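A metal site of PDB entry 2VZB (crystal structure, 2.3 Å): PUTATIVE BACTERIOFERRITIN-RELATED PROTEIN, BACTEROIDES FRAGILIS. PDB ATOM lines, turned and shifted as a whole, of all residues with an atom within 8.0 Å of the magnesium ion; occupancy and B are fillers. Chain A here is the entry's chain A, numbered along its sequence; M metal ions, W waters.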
ATOM      1  N   TYR A  36       1.006  -0.047  -5.939  1.00  0.00           N
ATOM      2  CA  TYR A  36       1.604  -1.367  -5.617  1.00  0.00           C
ATOM      3  C   TYR A  36       0.657  -2.532  -5.933  1.00  0.00           C
ATOM      4  O   TYR A  36       1.064  -3.573  -6.449  1.00  0.00           O
ATOM      5  CB  TYR A  36       1.954  -1.425  -4.147  1.00  0.00           C
ATOM      6  CG  TYR A  36       3.335  -0.959  -3.795  1.00  0.00           C
ATOM      7  CD1 TYR A  36       4.469  -1.492  -4.408  1.00  0.00           C
ATOM      8  CD2 TYR A  36       3.527  -0.005  -2.810  1.00  0.00           C
ATOM      9  CE1 TYR A  36       5.758  -1.084  -4.041  1.00  0.00           C
ATOM     10  CE2 TYR A  36       4.808   0.409  -2.440  1.00  0.00           C
ATOM     11  CZ  TYR A  36       5.900  -0.135  -3.068  1.00  0.00           C
ATOM     12  OH  TYR A  36       7.142   0.317  -2.700  1.00  0.00           O
ATOM     13  N   ASP A  50       9.175 -12.881  -6.601  1.00  0.00           N
ATOM     14  CA  ASP A  50       9.688 -12.059  -5.520  1.00  0.00           C
ATOM     15  C   ASP A  50       9.230 -10.609  -5.558  1.00  0.00           C
ATOM     16  O   ASP A  50       8.863 -10.049  -4.509  1.00  0.00           O
ATOM     17  CB  ASP A  50      11.214 -12.055  -5.529  1.00  0.00           C
ATOM     18  CG  ASP A  50      11.784 -13.397  -5.174  1.00  0.00           C
ATOM     19  OD1 ASP A  50      11.249 -14.076  -4.299  1.00  0.00           O
ATOM     20  OD2 ASP A  50      12.797 -13.784  -5.770  1.00  0.00           O
ATOM     21  N   GLY A  53       5.498 -10.387  -4.922  1.00  0.00           N
ATOM     22  CA  GLY A  53       5.365 -10.572  -3.493  1.00  0.00           C
ATOM     23  C   GLY A  53       5.631  -9.306  -2.695  1.00  0.00           C
ATOM     24  O   GLY A  53       4.855  -8.986  -1.802  1.00  0.00           O
ATOM     25  N   GLU A  54       6.702  -8.589  -3.013  1.00  0.00           N
ATOM     26  CA  GLU A  54       7.016  -7.318  -2.323  1.00  0.00           C
ATOM     27  C   GLU A  54       5.957  -6.286  -2.574  1.00  0.00           C
ATOM     28  O   GLU A  54       5.607  -5.549  -1.664  1.00  0.00           O
ATOM     29  CB  GLU A  54       8.316  -6.676  -2.775  1.00  0.00           C
ATOM     30  CG  GLU A  54       9.490  -7.504  -2.474  1.00  0.00           C
ATOM     31  CD  GLU A  54      10.105  -7.339  -1.127  1.00  0.00           C
ATOM     32  OE1 GLU A  54       9.789  -6.401  -0.361  1.00  0.00           O
ATOM     33  OE2 GLU A  54      10.953  -8.183  -0.830  1.00  0.00           O
ATOM     34  N   PHE A  55       5.500  -6.204  -3.822  1.00  0.00           N
ATOM     35  CA  PHE A  55       4.440  -5.240  -4.164  1.00  0.00           C
ATOM     36  C   PHE A  55       3.180  -5.490  -3.325  1.00  0.00           C
ATOM     37  O   PHE A  55       2.543  -4.572  -2.837  1.00  0.00           O
ATOM     38  CB  PHE A  55       4.088  -5.273  -5.660  1.00  0.00           C
ATOM     39  CG  PHE A  55       5.145  -4.669  -6.566  1.00  0.00           C
ATOM     40  CD1 PHE A  55       6.271  -4.024  -6.073  1.00  0.00           C
ATOM     41  CD2 PHE A  55       4.983  -4.717  -7.947  1.00  0.00           C
ATOM     42  CE1 PHE A  55       7.205  -3.486  -6.930  1.00  0.00           C
ATOM     43  CE2 PHE A  55       5.906  -4.173  -8.811  1.00  0.00           C
ATOM     44  CZ  PHE A  55       7.019  -3.553  -8.303  1.00  0.00           C
ATOM     45  N   GLU A  57       3.080  -7.086  -0.413  1.00  0.00           N
ATOM     46  CA  GLU A  57       3.400  -6.774   0.982  1.00  0.00           C
ATOM     47  C   GLU A  57       3.390  -5.265   1.225  1.00  0.00           C
ATOM     48  O   GLU A  57       2.836  -4.794   2.196  1.00  0.00           O
ATOM     49  CB  GLU A  57       4.739  -7.365   1.357  1.00  0.00           C
ATOM     50  CG  GLU A  57       4.730  -8.875   1.480  1.00  0.00           C
ATOM     51  CD  GLU A  57       6.128  -9.494   1.480  1.00  0.00           C
ATOM     52  OE1 GLU A  57       7.128  -8.758   1.412  1.00  0.00           O
ATOM     53  OE2 GLU A  57       6.241 -10.743   1.545  1.00  0.00           O
ATOM     54  N   HIS A  58       3.989  -4.529   0.304  1.00  0.00           N
ATOM     55  CA  HIS A  58       4.056  -3.071   0.392  1.00  0.00           C
ATOM     56  C   HIS A  58       2.683  -2.413   0.264  1.00  0.00           C
ATOM     57  O   HIS A  58       2.370  -1.462   0.986  1.00  0.00           O
ATOM     58  CB  HIS A  58       5.051  -2.527  -0.633  1.00  0.00           C
ATOM     59  CG  HIS A  58       6.469  -2.864  -0.310  1.00  0.00           C
ATOM     60  ND1 HIS A  58       7.544  -2.223  -0.895  1.00  0.00           N
ATOM     61  CD2 HIS A  58       7.002  -3.742   0.578  1.00  0.00           C
ATOM     62  CE1 HIS A  58       8.663  -2.728  -0.410  1.00  0.00           C
ATOM     63  NE2 HIS A  58       8.363  -3.644   0.493  1.00  0.00           N
ATOM     64  N   GLU A  61       1.268  -2.661   3.608  1.00  0.00           N
ATOM     65  CA  GLU A  61       1.931  -1.720   4.523  1.00  0.00           C
ATOM     66  C   GLU A  61       1.502  -0.262   4.332  1.00  0.00           C
ATOM     67  O   GLU A  61       1.296   0.452   5.299  1.00  0.00           O
ATOM     68  CB  GLU A  61       3.454  -1.897   4.461  1.00  0.00           C
ATOM     69  CG  GLU A  61       3.850  -3.235   5.130  1.00  0.00           C
ATOM     70  CD  GLU A  61       5.310  -3.602   5.020  1.00  0.00           C
ATOM     71  OE1 GLU A  61       6.030  -3.112   4.131  1.00  0.00           O
ATOM     72  OE2 GLU A  61       5.732  -4.431   5.848  1.00  0.00           O
ATOM     73  N   GLU A 145       9.522   2.577   7.682  1.00  0.00           N
ATOM     74  CA  GLU A 145       8.993   1.619   6.710  1.00  0.00           C
ATOM     75  C   GLU A 145       9.248   2.046   5.254  1.00  0.00           C
ATOM     76  O   GLU A 145       9.576   1.205   4.412  1.00  0.00           O
ATOM     77  CB  GLU A 145       7.500   1.327   6.949  1.00  0.00           C
ATOM     78  CG  GLU A 145       7.252   0.657   8.333  1.00  0.00           C
ATOM     79  CD  GLU A 145       5.945  -0.110   8.433  1.00  0.00           C
ATOM     80  OE1 GLU A 145       5.047   0.092   7.598  1.00  0.00           O
ATOM     81  OE2 GLU A 145       5.848  -0.918   9.386  1.00  0.00           O
ATOM     82  N   GLU A 148      12.732   1.331   4.303  1.00  0.00           N
ATOM     83  CA  GLU A 148      12.870  -0.125   4.074  1.00  0.00           C
ATOM     84  C   GLU A 148      12.325  -0.501   2.706  1.00  0.00           C
ATOM     85  O   GLU A 148      12.936  -1.295   1.986  1.00  0.00           O
ATOM     86  CB  GLU A 148      12.157  -0.940   5.170  1.00  0.00           C
ATOM     87  CG  GLU A 148      12.161  -2.461   4.906  1.00  0.00           C
ATOM     88  CD  GLU A 148      11.370  -3.219   5.973  1.00  0.00           C
ATOM     89  OE1 GLU A 148      10.441  -3.967   5.608  1.00  0.00           O
ATOM     90  OE2 GLU A 148      11.679  -3.020   7.159  1.00  0.00           O
ATOM     91  N   HIS A 149      11.164   0.040   2.362  1.00  0.00           N
ATOM     92  CA  HIS A 149      10.561  -0.177   1.039  1.00  0.00           C
ATOM     93  C   HIS A 149      11.518   0.228  -0.065  1.00  0.00           C
ATOM     94  O   HIS A 149      11.675  -0.506  -1.045  1.00  0.00           O
ATOM     95  CB  HIS A 149       9.293   0.663   0.833  1.00  0.00           C
ATOM     96  CG  HIS A 149       8.106   0.192   1.617  1.00  0.00           C
ATOM     97  ND1 HIS A 149       6.941   0.928   1.688  1.00  0.00           N
ATOM     98  CD2 HIS A 149       7.913  -0.915   2.376  1.00  0.00           C
ATOM     99  CE1 HIS A 149       6.078   0.282   2.444  1.00  0.00           C
ATOM    100  NE2 HIS A 149       6.638  -0.831   2.860  1.00  0.00           N
ATOM    101  N   GLU A 150      12.107   1.408   0.067  1.00  0.00           N
ATOM    102  CA  GLU A 150      13.094   1.881  -0.914  1.00  0.00           C
ATOM    103  C   GLU A 150      14.220   0.870  -1.072  1.00  0.00           C
ATOM    104  O   GLU A 150      14.544   0.470  -2.191  1.00  0.00           O
ATOM    105  CB  GLU A 150      13.712   3.263  -0.565  1.00  0.00           C
ATOM    106  CG  GLU A 150      14.368   3.864  -1.801  1.00  0.00           C
ATOM    107  CD  GLU A 150      15.520   4.832  -1.529  1.00  0.00           C
ATOM    108  OE1 GLU A 150      15.665   5.374  -0.395  1.00  0.00           O
ATOM    109  OE2 GLU A 150      16.273   5.058  -2.513  1.00  0.00           O
ATOM    110  N   GLN A 151      14.785   0.470   0.069  1.00  0.00           N
ATOM    111  CA  GLN A 151      15.868  -0.532   0.093  1.00  0.00           C
ATOM    112  C   GLN A 151      15.483  -1.837  -0.579  1.00  0.00           C
ATOM    113  O   GLN A 151      16.264  -2.396  -1.325  1.00  0.00           O
ATOM    114  CB  GLN A 151      16.280  -0.850   1.521  1.00  0.00           C
ATOM    115  CG  GLN A 151      17.471  -1.797   1.623  1.00  0.00           C
ATOM    116  CD  GLN A 151      18.724  -1.175   1.048  1.00  0.00           C
ATOM    117  OE1 GLN A 151      19.094  -0.075   1.422  1.00  0.00           O
ATOM    118  NE2 GLN A 151      19.379  -1.893   0.151  1.00  0.00           N
ATOM    119  N   ASP A 152      14.280  -2.320  -0.268  1.00  0.00           N
ATOM    120  CA  ASP A 152      13.783  -3.587  -0.836  1.00  0.00           C
ATOM    121  C   ASP A 152      13.755  -3.513  -2.366  1.00  0.00           C
ATOM    122  O   ASP A 152      14.113  -4.462  -3.052  1.00  0.00           O
ATOM    123  CB  ASP A 152      12.370  -3.893  -0.317  1.00  0.00           C
ATOM    124  CG  ASP A 152      12.310  -4.207   1.193  1.00  0.00           C
ATOM    125  OD1 ASP A 152      13.339  -4.574   1.800  1.00  0.00           O
ATOM    126  OD2 ASP A 152      11.196  -4.094   1.740  1.00  0.00           O
ATOM    127  N   LEU A 153      13.269  -2.386  -2.878  1.00  0.00           N
ATOM    128  CA  LEU A 153      13.079  -2.231  -4.312  1.00  0.00           C
ATOM    129  C   LEU A 153      14.444  -2.054  -5.004  1.00  0.00           C
ATOM    130  O   LEU A 153      14.730  -2.659  -6.010  1.00  0.00           O
ATOM    131  CB  LEU A 153      12.150  -1.038  -4.609  1.00  0.00           C
ATOM    132  CG  LEU A 153      10.715  -1.174  -4.103  1.00  0.00           C
ATOM    133  CD1 LEU A 153       9.882  -0.012  -4.574  1.00  0.00           C
ATOM    134  CD2 LEU A 153      10.071  -2.470  -4.534  1.00  0.00           C
ATOM    135  N   TYR A 156      16.319  -5.307  -5.697  1.00  0.00           N
ATOM    136  CA  TYR A 156      15.928  -6.024  -6.921  1.00  0.00           C
ATOM    137  C   TYR A 156      16.555  -5.395  -8.176  1.00  0.00           C
ATOM    138  O   TYR A 156      17.037  -6.103  -9.054  1.00  0.00           O
ATOM    139  CB  TYR A 156      14.416  -6.104  -7.097  1.00  0.00           C
ATOM    140  CG  TYR A 156      13.732  -6.952  -6.059  1.00  0.00           C
ATOM    141  CD1 TYR A 156      13.997  -8.330  -5.947  1.00  0.00           C
ATOM    142  CD2 TYR A 156      12.812  -6.397  -5.200  1.00  0.00           C
ATOM    143  CE1 TYR A 156      13.368  -9.097  -4.982  1.00  0.00           C
ATOM    144  CE2 TYR A 156      12.171  -7.135  -4.250  1.00  0.00           C
ATOM    145  CZ  TYR A 156      12.440  -8.490  -4.138  1.00  0.00           C
ATOM    146  OH  TYR A 156      11.778  -9.207  -3.156  1.00  0.00           O
HETATM  147 MG    MG M   1       9.403  -5.220   1.744  1.00  0.00          MG
HETATM  148  O   HOH W   1       7.834  -6.438   2.321  1.00  0.00           O
HETATM  149  O   HOH W   2      10.539  -6.394   3.369  1.00  0.00           O
HETATM  150  O   HOH W   3       8.725  -4.124   3.315  1.00  0.00           O
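OH of Tyr 36 sits at hydrogen-bond distance from ND1 of His 58 (3.1 Å).
OH of Tyr 156 sits at hydrogen-bond distance from OE2 of Glu 54 (2.7 Å).
Within 4 Å of the magnesium ion: Glu 54, His 58 and Asp 152.
The nearest printed residue that does not touch the magnesium ion is Glu 148 (4.2 Å).
The magnesium ion is bound by water W3 (2.0 Å), water W1 (2.1 Å), OD2 of Asp 152 (2.1 Å), NE2 of His 58 (2.3 Å), water W2 (2.3 Å) and OE1 of Glu 54 (2.4 Å).
Water W3 lies within hydrogen-bond range of the side-chain carboxylate (OE1) of Glu 148 and the side-chain carboxylate (OE1) of Glu 61.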
